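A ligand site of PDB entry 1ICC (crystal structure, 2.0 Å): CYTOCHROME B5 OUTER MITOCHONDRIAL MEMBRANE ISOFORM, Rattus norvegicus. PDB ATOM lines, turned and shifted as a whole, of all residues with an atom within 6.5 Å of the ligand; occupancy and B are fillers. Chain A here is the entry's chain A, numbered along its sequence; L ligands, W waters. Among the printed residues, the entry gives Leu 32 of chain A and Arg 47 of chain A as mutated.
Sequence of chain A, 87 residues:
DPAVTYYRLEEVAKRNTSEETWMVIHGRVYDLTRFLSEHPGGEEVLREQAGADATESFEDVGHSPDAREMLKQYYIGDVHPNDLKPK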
ATOM      1  N   MET A  23     -12.525 -22.625  18.383  1.00  0.00           N
ATOM      2  CA  MET A  23     -11.207 -22.144  18.006  1.00  0.00           C
ATOM      3  C   MET A  23     -10.182 -23.086  18.638  1.00  0.00           C
ATOM      4  O   MET A  23     -10.395 -23.611  19.741  1.00  0.00           O
ATOM      5  CB  MET A  23     -11.056 -20.683  18.508  1.00  0.00           C
ATOM      6  CG  MET A  23      -9.735 -20.009  18.160  1.00  0.00           C
ATOM      7  SD  MET A  23      -9.705 -18.274  18.769  1.00  0.00           S
ATOM      8  CE  MET A  23     -10.938 -17.520  17.704  1.00  0.00           C
ATOM      9  N   ILE A  25      -6.413 -23.635  20.215  1.00  0.00           N
ATOM     10  CA  ILE A  25      -5.306 -22.937  20.924  1.00  0.00           C
ATOM     11  C   ILE A  25      -4.419 -24.046  21.536  1.00  0.00           C
ATOM     12  O   ILE A  25      -4.920 -24.868  22.320  1.00  0.00           O
ATOM     13  CB  ILE A  25      -5.828 -22.070  22.091  1.00  0.00           C
ATOM     14  CG1 ILE A  25      -6.821 -20.998  21.600  1.00  0.00           C
ATOM     15  CG2 ILE A  25      -4.629 -21.395  22.818  1.00  0.00           C
ATOM     16  CD1 ILE A  25      -6.152 -19.878  20.859  1.00  0.00           C
ATOM     17  N   TYR A  30     -11.801 -25.042  21.748  1.00  0.00           N
ATOM     18  CA  TYR A  30     -12.581 -24.236  22.656  1.00  0.00           C
ATOM     19  C   TYR A  30     -13.856 -23.745  22.046  1.00  0.00           C
ATOM     20  O   TYR A  30     -13.844 -23.191  20.947  1.00  0.00           O
ATOM     21  CB  TYR A  30     -11.722 -23.040  23.086  1.00  0.00           C
ATOM     22  CG  TYR A  30     -10.487 -23.455  23.881  1.00  0.00           C
ATOM     23  CD1 TYR A  30      -9.278 -23.754  23.231  1.00  0.00           C
ATOM     24  CD2 TYR A  30     -10.551 -23.591  25.265  1.00  0.00           C
ATOM     25  CE1 TYR A  30      -8.177 -24.179  23.961  1.00  0.00           C
ATOM     26  CE2 TYR A  30      -9.464 -24.005  26.010  1.00  0.00           C
ATOM     27  CZ  TYR A  30      -8.281 -24.304  25.350  1.00  0.00           C
ATOM     28  OH  TYR A  30      -7.242 -24.775  26.096  1.00  0.00           O
ATOM     29  N   LEU A  32     -16.022 -21.031  22.059  1.00  0.00           N
ATOM     30  CA  LEU A  32     -16.104 -19.644  22.530  1.00  0.00           C
ATOM     31  C   LEU A  32     -17.426 -18.950  22.174  1.00  0.00           C
ATOM     32  O   LEU A  32     -17.549 -17.732  22.273  1.00  0.00           O
ATOM     33  CB  LEU A  32     -14.942 -18.832  21.946  1.00  0.00           C
ATOM     34  CG  LEU A  32     -13.547 -19.440  22.170  1.00  0.00           C
ATOM     35  CD1 LEU A  32     -12.493 -18.645  21.317  1.00  0.00           C
ATOM     36  CD2 LEU A  32     -13.202 -19.371  23.679  1.00  0.00           C
ATOM     37  N   PHE A  35     -18.388 -16.707  24.757  1.00  0.00           N
ATOM     38  CA  PHE A  35     -17.312 -15.792  25.161  1.00  0.00           C
ATOM     39  C   PHE A  35     -17.209 -14.574  24.252  1.00  0.00           C
ATOM     40  O   PHE A  35     -16.720 -13.554  24.680  1.00  0.00           O
ATOM     41  CB  PHE A  35     -15.957 -16.519  25.117  1.00  0.00           C
ATOM     42  CG  PHE A  35     -14.767 -15.618  25.401  1.00  0.00           C
ATOM     43  CD1 PHE A  35     -14.623 -14.993  26.630  1.00  0.00           C
ATOM     44  CD2 PHE A  35     -13.788 -15.393  24.432  1.00  0.00           C
ATOM     45  CE1 PHE A  35     -13.552 -14.168  26.902  1.00  0.00           C
ATOM     46  CE2 PHE A  35     -12.680 -14.529  24.708  1.00  0.00           C
ATOM     47  CZ  PHE A  35     -12.588 -13.941  25.949  1.00  0.00           C
ATOM     48  N   GLU A  38     -17.797 -10.992  25.560  1.00  0.00           N
ATOM     49  CA  GLU A  38     -16.981 -10.582  26.674  1.00  0.00           C
ATOM     50  C   GLU A  38     -15.484 -10.468  26.432  1.00  0.00           C
ATOM     51  O   GLU A  38     -14.734 -10.190  27.376  1.00  0.00           O
ATOM     52  CB  GLU A  38     -17.221 -11.555  27.816  1.00  0.00           C
ATOM     53  CG  GLU A  38     -18.728 -11.726  28.098  1.00  0.00           C
ATOM     54  CD  GLU A  38     -19.439 -10.382  28.242  1.00  0.00           C
ATOM     55  OE1 GLU A  38     -18.840  -9.469  28.881  1.00  0.00           O
ATOM     56  OE2 GLU A  38     -20.588 -10.250  27.713  1.00  0.00           O
ATOM     57  N   HIS A  39     -15.059 -10.646  25.172  1.00  0.00           N
ATOM     58  CA  HIS A  39     -13.642 -10.596  24.848  1.00  0.00           C
ATOM     59  C   HIS A  39     -13.178  -9.143  24.782  1.00  0.00           C
ATOM     60  O   HIS A  39     -13.623  -8.383  23.908  1.00  0.00           O
ATOM     61  CB  HIS A  39     -13.404 -11.246  23.499  1.00  0.00           C
ATOM     62  CG  HIS A  39     -11.991 -11.167  23.024  1.00  0.00           C
ATOM     63  ND1 HIS A  39     -11.650 -10.730  21.768  1.00  0.00           N
ATOM     64  CD2 HIS A  39     -10.837 -11.462  23.648  1.00  0.00           C
ATOM     65  CE1 HIS A  39     -10.337 -10.751  21.630  1.00  0.00           C
ATOM     66  NE2 HIS A  39      -9.823 -11.191  22.759  1.00  0.00           N
ATOM     67  N   PRO A  40     -12.235  -8.746  25.674  1.00  0.00           N
ATOM     68  CA  PRO A  40     -11.764  -7.359  25.664  1.00  0.00           C
ATOM     69  C   PRO A  40     -11.204  -6.866  24.327  1.00  0.00           C
ATOM     70  O   PRO A  40     -11.293  -5.652  24.024  1.00  0.00           O
ATOM     71  CB  PRO A  40     -10.733  -7.338  26.792  1.00  0.00           C
ATOM     72  CG  PRO A  40     -11.213  -8.379  27.722  1.00  0.00           C
ATOM     73  CD  PRO A  40     -11.568  -9.509  26.729  1.00  0.00           C
ATOM     74  N   GLY A  41     -10.631  -7.774  23.541  1.00  0.00           N
ATOM     75  CA  GLY A  41     -10.117  -7.387  22.240  1.00  0.00           C
ATOM     76  C   GLY A  41     -11.226  -7.229  21.185  1.00  0.00           C
ATOM     77  O   GLY A  41     -10.949  -6.903  20.006  1.00  0.00           O
ATOM     78  N   GLY A  42     -12.467  -7.491  21.582  1.00  0.00           N
ATOM     79  CA  GLY A  42     -13.598  -7.339  20.688  1.00  0.00           C
ATOM     80  C   GLY A  42     -13.965  -8.600  19.935  1.00  0.00           C
ATOM     81  O   GLY A  42     -13.205  -9.593  19.932  1.00  0.00           O
ATOM     82  N   VAL A  45     -11.864  -9.692  15.859  1.00  0.00           N
ATOM     83  CA  VAL A  45     -10.642 -10.499  15.766  1.00  0.00           C
ATOM     84  C   VAL A  45     -10.901 -11.962  16.052  1.00  0.00           C
ATOM     85  O   VAL A  45     -10.128 -12.819  15.625  1.00  0.00           O
ATOM     86  CB  VAL A  45      -9.522  -9.967  16.674  1.00  0.00           C
ATOM     87  CG1 VAL A  45      -9.145  -8.595  16.185  1.00  0.00           C
ATOM     88  CG2 VAL A  45      -9.936  -9.982  18.159  1.00  0.00           C
ATOM     89  N   LEU A  46     -11.977 -12.265  16.763  1.00  0.00           N
ATOM     90  CA  LEU A  46     -12.272 -13.658  17.027  1.00  0.00           C
ATOM     91  C   LEU A  46     -13.007 -14.190  15.813  1.00  0.00           C
ATOM     92  O   LEU A  46     -12.713 -15.311  15.368  1.00  0.00           O
ATOM     93  CB  LEU A  46     -13.106 -13.875  18.304  1.00  0.00           C
ATOM     94  CG  LEU A  46     -12.503 -13.370  19.627  1.00  0.00           C
ATOM     95  CD1 LEU A  46     -13.396 -13.779  20.844  1.00  0.00           C
ATOM     96  CD2 LEU A  46     -11.075 -13.975  19.773  1.00  0.00           C
ATOM     97  N   ARG A  47     -13.949 -13.418  15.234  1.00  0.00           N
ATOM     98  CA  ARG A  47     -14.650 -13.938  14.049  1.00  0.00           C
ATOM     99  C   ARG A  47     -13.620 -14.277  12.955  1.00  0.00           C
ATOM    100  O   ARG A  47     -13.723 -15.319  12.309  1.00  0.00           O
ATOM    101  CB  ARG A  47     -15.677 -12.933  13.456  1.00  0.00           C
ATOM    102  CG  ARG A  47     -16.753 -12.453  14.408  1.00  0.00           C
ATOM    103  CD  ARG A  47     -17.631 -11.335  13.791  1.00  0.00           C
ATOM    104  NE  ARG A  47     -18.567 -10.807  14.791  1.00  0.00           N
ATOM    105  CZ  ARG A  47     -18.802  -9.518  14.974  1.00  0.00           C
ATOM    106  NH1 ARG A  47     -18.168  -8.618  14.240  1.00  0.00           N
ATOM    107  NH2 ARG A  47     -19.707  -9.129  15.885  1.00  0.00           N
ATOM    108  N   GLU A  48     -12.633 -13.406  12.761  1.00  0.00           N
ATOM    109  CA  GLU A  48     -11.607 -13.600  11.714  1.00  0.00           C
ATOM    110  C   GLU A  48     -10.942 -14.970  11.730  1.00  0.00           C
ATOM    111  O   GLU A  48     -10.520 -15.480  10.709  1.00  0.00           O
ATOM    112  CB  GLU A  48     -10.451 -12.568  11.862  1.00  0.00           C
ATOM    113  CG  GLU A  48     -10.886 -11.106  11.866  1.00  0.00           C
ATOM    114  CD  GLU A  48      -9.723 -10.084  11.764  1.00  0.00           C
ATOM    115  OE1 GLU A  48      -8.650 -10.276  12.382  1.00  0.00           O
ATOM    116  OE2 GLU A  48      -9.931  -9.059  11.057  1.00  0.00           O
ATOM    117  N   GLN A  49     -10.768 -15.523  12.917  1.00  0.00           N
ATOM    118  CA  GLN A  49     -10.133 -16.801  13.058  1.00  0.00           C
ATOM    119  C   GLN A  49     -10.981 -17.906  13.644  1.00  0.00           C
ATOM    120  O   GLN A  49     -10.473 -18.927  14.046  1.00  0.00           O
ATOM    121  CB  GLN A  49      -8.859 -16.623  13.874  1.00  0.00           C
ATOM    122  CG  GLN A  49      -7.768 -16.044  12.987  1.00  0.00           C
ATOM    123  CD  GLN A  49      -6.489 -15.892  13.738  1.00  0.00           C
ATOM    124  OE1 GLN A  49      -6.245 -14.867  14.361  1.00  0.00           O
ATOM    125  NE2 GLN A  49      -5.679 -16.919  13.706  1.00  0.00           N
ATOM    126  N   ALA A  50     -12.284 -17.724  13.670  1.00  0.00           N
ATOM    127  CA  ALA A  50     -13.133 -18.754  14.186  1.00  0.00           C
ATOM    128  C   ALA A  50     -13.021 -19.957  13.269  1.00  0.00           C
ATOM    129  O   ALA A  50     -12.916 -19.819  12.041  1.00  0.00           O
ATOM    130  CB  ALA A  50     -14.550 -18.275  14.227  1.00  0.00           C
ATOM    131  N   ALA A  54      -5.820 -20.577  16.334  1.00  0.00           N
ATOM    132  CA  ALA A  54      -5.425 -19.179  16.429  1.00  0.00           C
ATOM    133  C   ALA A  54      -4.301 -19.018  17.468  1.00  0.00           C
ATOM    134  O   ALA A  54      -4.095 -17.926  18.037  1.00  0.00           O
ATOM    135  CB  ALA A  54      -6.648 -18.338  16.812  1.00  0.00           C
ATOM    136  N   SER A  57      -1.889 -15.992  16.787  1.00  0.00           N
ATOM    137  CA  SER A  57      -2.406 -14.655  17.069  1.00  0.00           C
ATOM    138  C   SER A  57      -2.552 -14.507  18.576  1.00  0.00           C
ATOM    139  O   SER A  57      -2.185 -13.493  19.129  1.00  0.00           O
ATOM    140  CB  SER A  57      -3.746 -14.407  16.393  1.00  0.00           C
ATOM    141  OG  SER A  57      -3.598 -14.516  14.991  1.00  0.00           O
ATOM    142  N   PHE A  58      -3.066 -15.530  19.227  1.00  0.00           N
ATOM    143  CA  PHE A  58      -3.233 -15.487  20.673  1.00  0.00           C
ATOM    144  C   PHE A  58      -1.907 -15.140  21.370  1.00  0.00           C
ATOM    145  O   PHE A  58      -1.834 -14.242  22.211  1.00  0.00           O
ATOM    146  CB  PHE A  58      -3.709 -16.833  21.179  1.00  0.00           C
ATOM    147  CG  PHE A  58      -4.048 -16.834  22.632  1.00  0.00           C
ATOM    148  CD1 PHE A  58      -5.278 -16.361  23.063  1.00  0.00           C
ATOM    149  CD2 PHE A  58      -3.153 -17.375  23.571  1.00  0.00           C
ATOM    150  CE1 PHE A  58      -5.643 -16.411  24.379  1.00  0.00           C
ATOM    151  CE2 PHE A  58      -3.512 -17.432  24.929  1.00  0.00           C
ATOM    152  CZ  PHE A  58      -4.753 -16.961  25.332  1.00  0.00           C
ATOM    153  N   VAL A  61      -0.412 -11.446  20.572  1.00  0.00           N
ATOM    154  CA  VAL A  61      -1.098 -10.343  21.229  1.00  0.00           C
ATOM    155  C   VAL A  61      -0.540 -10.201  22.636  1.00  0.00           C
ATOM    156  O   VAL A  61      -0.468  -9.104  23.194  1.00  0.00           O
ATOM    157  CB  VAL A  61      -2.651 -10.584  21.242  1.00  0.00           C
ATOM    158  CG1 VAL A  61      -3.285  -9.894  22.402  1.00  0.00           C
ATOM    159  CG2 VAL A  61      -3.261 -10.073  19.942  1.00  0.00           C
ATOM    160  N   GLY A  62      -0.127 -11.324  23.224  1.00  0.00           N
ATOM    161  CA  GLY A  62       0.434 -11.277  24.572  1.00  0.00           C
ATOM    162  C   GLY A  62      -0.606 -11.338  25.685  1.00  0.00           C
ATOM    163  O   GLY A  62      -0.594 -10.482  26.596  1.00  0.00           O
ATOM    164  N   HIS A  63      -1.482 -12.342  25.638  1.00  0.00           N
ATOM    165  CA  HIS A  63      -2.486 -12.482  26.666  1.00  0.00           C
ATOM    166  C   HIS A  63      -1.921 -12.743  28.053  1.00  0.00           C
ATOM    167  O   HIS A  63      -0.953 -13.489  28.232  1.00  0.00           O
ATOM    168  CB  HIS A  63      -3.473 -13.588  26.303  1.00  0.00           C
ATOM    169  CG  HIS A  63      -4.348 -13.256  25.154  1.00  0.00           C
ATOM    170  ND1 HIS A  63      -3.926 -13.357  23.846  1.00  0.00           N
ATOM    171  CD2 HIS A  63      -5.604 -12.760  25.107  1.00  0.00           C
ATOM    172  CE1 HIS A  63      -4.895 -12.933  23.042  1.00  0.00           C
ATOM    173  NE2 HIS A  63      -5.921 -12.573  23.787  1.00  0.00           N
ATOM    174  N   SER A  64      -2.571 -12.108  29.018  1.00  0.00           N
ATOM    175  CA  SER A  64      -2.218 -12.178  30.436  1.00  0.00           C
ATOM    176  C   SER A  64      -2.508 -13.510  31.082  1.00  0.00           C
ATOM    177  O   SER A  64      -3.237 -14.320  30.531  1.00  0.00           O
ATOM    178  CB  SER A  64      -3.032 -11.152  31.192  1.00  0.00           C
ATOM    179  OG  SER A  64      -4.341 -11.653  31.459  1.00  0.00           O
ATOM    180  N   PRO A  65      -1.967 -13.735  32.293  1.00  0.00           N
ATOM    181  CA  PRO A  65      -2.217 -14.991  33.027  1.00  0.00           C
ATOM    182  C   PRO A  65      -3.737 -15.208  33.230  1.00  0.00           C
ATOM    183  O   PRO A  65      -4.248 -16.332  33.120  1.00  0.00           O
ATOM    184  CB  PRO A  65      -1.513 -14.758  34.380  1.00  0.00           C
ATOM    185  CG  PRO A  65      -0.433 -13.814  34.025  1.00  0.00           C
ATOM    186  CD  PRO A  65      -0.994 -12.872  32.990  1.00  0.00           C
ATOM    187  N   ASP A  66      -4.467 -14.151  33.540  1.00  0.00           N
ATOM    188  CA  ASP A  66      -5.909 -14.309  33.763  1.00  0.00           C
ATOM    189  C   ASP A  66      -6.631 -14.647  32.467  1.00  0.00           C
ATOM    190  O   ASP A  66      -7.654 -15.337  32.512  1.00  0.00           O
ATOM    191  CB  ASP A  66      -6.517 -13.049  34.400  1.00  0.00           C
ATOM    192  CG  ASP A  66      -5.929 -12.770  35.776  1.00  0.00           C
ATOM    193  OD1 ASP A  66      -5.915 -13.706  36.630  1.00  0.00           O
ATOM    194  OD2 ASP A  66      -5.494 -11.625  35.991  1.00  0.00           O
ATOM    195  N   ALA A  67      -6.103 -14.165  31.349  1.00  0.00           N
ATOM    196  CA  ALA A  67      -6.671 -14.490  30.032  1.00  0.00           C
ATOM    197  C   ALA A  67      -6.462 -15.964  29.786  1.00  0.00           C
ATOM    198  O   ALA A  67      -7.342 -16.655  29.267  1.00  0.00           O
ATOM    199  CB  ALA A  67      -5.978 -13.742  28.928  1.00  0.00           C
ATOM    200  N   ARG A  68      -5.293 -16.460  30.158  1.00  0.00           N
ATOM    201  CA  ARG A  68      -5.076 -17.875  29.894  1.00  0.00           C
ATOM    202  C   ARG A  68      -5.972 -18.690  30.825  1.00  0.00           C
ATOM    203  O   ARG A  68      -6.507 -19.696  30.414  1.00  0.00           O
ATOM    204  CB  ARG A  68      -3.604 -18.248  30.082  1.00  0.00           C
ATOM    205  CG  ARG A  68      -2.672 -17.437  29.245  1.00  0.00           C
ATOM    206  CD  ARG A  68      -1.267 -17.938  29.425  1.00  0.00           C
ATOM    207  NE  ARG A  68      -0.353 -17.132  28.650  1.00  0.00           N
ATOM    208  CZ  ARG A  68       0.078 -17.438  27.428  1.00  0.00           C
ATOM    209  NH1 ARG A  68      -0.327 -18.546  26.821  1.00  0.00           N
ATOM    210  NH2 ARG A  68       0.941 -16.626  26.823  1.00  0.00           N
ATOM    211  N   MET A  70      -8.928 -17.997  31.783  1.00  0.00           N
ATOM    212  CA  MET A  70     -10.262 -17.883  31.200  1.00  0.00           C
ATOM    213  C   MET A  70     -10.536 -18.933  30.126  1.00  0.00           C
ATOM    214  O   MET A  70     -11.699 -19.236  29.803  1.00  0.00           O
ATOM    215  CB  MET A  70     -10.381 -16.503  30.574  1.00  0.00           C
ATOM    216  CG  MET A  70     -11.645 -15.800  30.853  1.00  0.00           C
ATOM    217  SD  MET A  70     -11.633 -14.174  30.105  1.00  0.00           S
ATOM    218  CE  MET A  70     -11.258 -13.084  31.481  1.00  0.00           C
ATOM    219  N   LEU A  71      -9.463 -19.472  29.557  1.00  0.00           N
ATOM    220  CA  LEU A  71      -9.603 -20.474  28.513  1.00  0.00           C
ATOM    221  C   LEU A  71     -10.221 -21.759  28.975  1.00  0.00           C
ATOM    222  O   LEU A  71     -11.009 -22.380  28.241  1.00  0.00           O
ATOM    223  CB  LEU A  71      -8.239 -20.842  27.967  1.00  0.00           C
ATOM    224  CG  LEU A  71      -7.723 -20.011  26.810  1.00  0.00           C
ATOM    225  CD1 LEU A  71      -6.307 -20.470  26.520  1.00  0.00           C
ATOM    226  CD2 LEU A  71      -8.598 -20.218  25.566  1.00  0.00           C
ATOM    227  N   LYS A  72      -9.861 -22.146  30.194  1.00  0.00           N
ATOM    228  CA  LYS A  72     -10.301 -23.412  30.723  1.00  0.00           C
ATOM    229  C   LYS A  72     -11.777 -23.719  30.699  1.00  0.00           C
ATOM    230  O   LYS A  72     -12.184 -24.817  30.330  1.00  0.00           O
ATOM    231  CB  LYS A  72      -9.744 -23.591  32.131  1.00  0.00           C
ATOM    232  CG  LYS A  72      -8.214 -23.484  32.190  1.00  0.00           C
ATOM    233  CD  LYS A  72      -7.715 -23.718  33.624  1.00  0.00           C
ATOM    234  CE  LYS A  72      -6.235 -23.543  33.763  1.00  0.00           C
ATOM    235  NZ  LYS A  72      -5.914 -23.528  35.220  1.00  0.00           N
ATOM    236  N   GLN A  73     -12.590 -22.745  31.059  1.00  0.00           N
ATOM    237  CA  GLN A  73     -14.018 -22.979  31.087  1.00  0.00           C
ATOM    238  C   GLN A  73     -14.602 -23.310  29.702  1.00  0.00           C
ATOM    239  O   GLN A  73     -15.700 -23.887  29.619  1.00  0.00           O
ATOM    240  CB  GLN A  73     -14.748 -21.760  31.668  1.00  0.00           C
ATOM    241  CG  GLN A  73     -14.742 -20.578  30.768  1.00  0.00           C
ATOM    242  CD  GLN A  73     -15.126 -19.291  31.475  1.00  0.00           C
ATOM    243  OE1 GLN A  73     -16.240 -19.150  31.956  1.00  0.00           O
ATOM    244  NE2 GLN A  73     -14.171 -18.329  31.536  1.00  0.00           N
ATOM    245  N   TYR A  74     -13.893 -22.952  28.628  1.00  0.00           N
ATOM    246  CA  TYR A  74     -14.403 -23.221  27.284  1.00  0.00           C
ATOM    247  C   TYR A  74     -13.774 -24.426  26.582  1.00  0.00           C
ATOM    248  O   TYR A  74     -14.090 -24.690  25.398  1.00  0.00           O
ATOM    249  CB  TYR A  74     -14.261 -21.993  26.391  1.00  0.00           C
ATOM    250  CG  TYR A  74     -14.857 -20.737  27.002  1.00  0.00           C
ATOM    251  CD1 TYR A  74     -16.229 -20.626  27.222  1.00  0.00           C
ATOM    252  CD2 TYR A  74     -14.028 -19.681  27.410  1.00  0.00           C
ATOM    253  CE1 TYR A  74     -16.771 -19.512  27.831  1.00  0.00           C
ATOM    254  CE2 TYR A  74     -14.571 -18.526  28.039  1.00  0.00           C
ATOM    255  CZ  TYR A  74     -15.933 -18.468  28.236  1.00  0.00           C
ATOM    256  OH  TYR A  74     -16.487 -17.355  28.818  1.00  0.00           O
HETATM  257  C1  LIG L   1      -7.345  -8.889  25.090  1.00  0.00           C
HETATM  258  C2  LIG L   1      -6.842 -10.536  20.591  1.00  0.00           C
HETATM  259  C3  LIG L   1      -8.440 -14.890  21.873  1.00  0.00           C
HETATM  260  C4  LIG L   1      -9.036 -13.261  26.357  1.00  0.00           C
HETATM  261  C5  LIG L   1      -7.078  -8.949  23.734  1.00  0.00           C
HETATM  262  C6  LIG L   1      -6.607  -7.874  22.967  1.00  0.00           C
HETATM  263  C7  LIG L   1      -6.466  -8.346  21.667  1.00  0.00           C
HETATM  264  C8  LIG L   1      -6.864  -9.716  21.668  1.00  0.00           C
HETATM  265  C9  LIG L   1      -6.002  -7.590  20.557  1.00  0.00           C
HETATM  266  C10 LIG L   1      -6.273  -6.450  23.474  1.00  0.00           C
HETATM  267  C11 LIG L   1      -4.771  -6.188  23.707  1.00  0.00           C
HETATM  268  C12 LIG L   1      -4.495  -5.356  24.934  1.00  0.00           C
HETATM  269  O1  LIG L   1      -4.759  -5.837  26.065  1.00  0.00           O
HETATM  270  O2  LIG L   1      -3.994  -4.226  24.746  1.00  0.00           O
HETATM  271  C13 LIG L   1      -7.220 -11.868  20.581  1.00  0.00           C
HETATM  272  C14 LIG L   1      -7.155 -12.709  19.400  1.00  0.00           C
HETATM  273  C15 LIG L   1      -7.589 -13.951  19.721  1.00  0.00           C
HETATM  274  C16 LIG L   1      -7.941 -13.833  21.150  1.00  0.00           C
HETATM  275  C17 LIG L   1      -6.652 -12.204  18.053  1.00  0.00           C
HETATM  276  C18 LIG L   1      -7.691 -15.143  18.835  1.00  0.00           C
HETATM  277  C19 LIG L   1      -8.450 -14.958  17.541  1.00  0.00           C
HETATM  278  C20 LIG L   1      -8.761 -14.821  23.196  1.00  0.00           C
HETATM  279  C21 LIG L   1      -9.291 -15.942  23.989  1.00  0.00           C
HETATM  280  C22 LIG L   1      -9.444 -15.502  25.263  1.00  0.00           C
HETATM  281  C23 LIG L   1      -9.035 -14.092  25.256  1.00  0.00           C
HETATM  282  C24 LIG L   1      -9.593 -17.367  23.480  1.00  0.00           C
HETATM  283  C25 LIG L   1      -9.895 -16.301  26.468  1.00  0.00           C
HETATM  284  C26 LIG L   1     -11.083 -16.847  26.722  1.00  0.00           C
HETATM  285  C27 LIG L   1      -8.621 -11.937  26.406  1.00  0.00           C
HETATM  286  C28 LIG L   1      -8.618 -11.116  27.625  1.00  0.00           C
HETATM  287  C29 LIG L   1      -8.124  -9.898  27.271  1.00  0.00           C
HETATM  288  C30 LIG L   1      -7.847  -9.975  25.837  1.00  0.00           C
HETATM  289  C31 LIG L   1      -9.066 -11.517  29.040  1.00  0.00           C
HETATM  290  C32 LIG L   1      -7.886  -8.698  28.199  1.00  0.00           C
HETATM  291  C33 LIG L   1      -6.333  -8.502  28.383  1.00  0.00           C
HETATM  292  C34 LIG L   1      -5.614  -9.695  28.993  1.00  0.00           C
HETATM  293  O3  LIG L   1      -4.565 -10.142  28.428  1.00  0.00           O
HETATM  294  O4  LIG L   1      -6.109 -10.175  30.032  1.00  0.00           O
HETATM  295  N1  LIG L   1      -7.258 -10.100  22.942  1.00  0.00           N
HETATM  296  N2  LIG L   1      -7.689 -12.556  21.667  1.00  0.00           N
HETATM  297  N3  LIG L   1      -8.604 -13.669  23.986  1.00  0.00           N
HETATM  298  N4  LIG L   1      -8.151 -11.220  25.317  1.00  0.00           N
HETATM  299 FE1  LIG L   1      -7.939 -11.857  23.493  1.00  0.00          FE
HETATM  300  O   HOH W   1      -7.675  -9.048  31.808  1.00  0.00           O
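An iron atom (FE1) of the ligand is bound by a ring nitrogen (NE2) of His 39 (2.1 Å). The side-chain hydroxyl (OG) of Ser 64 lies within hydrogen-bond range of an oxygen (O4) of the ligand, 2.7 Å away. O3 of the ligand sits at hydrogen-bond distance from N of Ser 64, 2.9 Å away. A ring nitrogen (NE2) of His 63 is bound to an iron atom (FE1) of the ligand, at 2.2 Å.
A ring nitrogen (ND1) of His 39 sits at hydrogen-bond distance from the backbone carbonyl oxygen of Gly 42 (2.7 Å). OE1 of Gln 49 lies within hydrogen-bond range of OG of Ser 57. The backbone NH of Tyr 30 is in hydrogen-bond range of the backbone carbonyl oxygen of Met 23 (2.8 Å). The backbone NH (N) of Asp 66 sits close to the side-chain hydroxyl (OG) of Ser 64, 3.3 Å away. N of Ala 67 sits at hydrogen-bond distance from OG of Ser 64 (3.1 Å). A ring nitrogen (ND1) of His 63 lies within hydrogen-bond range of the backbone carbonyl oxygen of Phe 58, 2.8 Å away. The backbone carbonyl oxygen (O) of Met 70 sits at hydrogen-bond distance from the side-chain amide nitrogen (NE2) of Gln 73, at 3.2 Å.
Merely in contact with the ligand: Val 45, Phe 35, Pro 40, Leu 46, Met 23, Val 61, Gly 41, Met 70, Leu 71, Phe 58, Ala 67, Leu 32, Gln 49 and Ala 54. Hydrophobic or aromatic side chains that line the ligand: Met 23, Leu 32, Phe 35, His 39, Pro 40, Val 45, Leu 46, Ala 54, Phe 58, Val 61, His 63, Ala 67, Met 70 and Leu 71. 17 residues have an atom within 4 Å of the ligand: Met 23, Leu 32, Phe 35, His 39, Pro 40, Gly 41, Val 45, Leu 46, Gln 49, Ala 54, Phe 58, Val 61, His 63, Ser 64, Ala 67, Met 70 and Leu 71.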
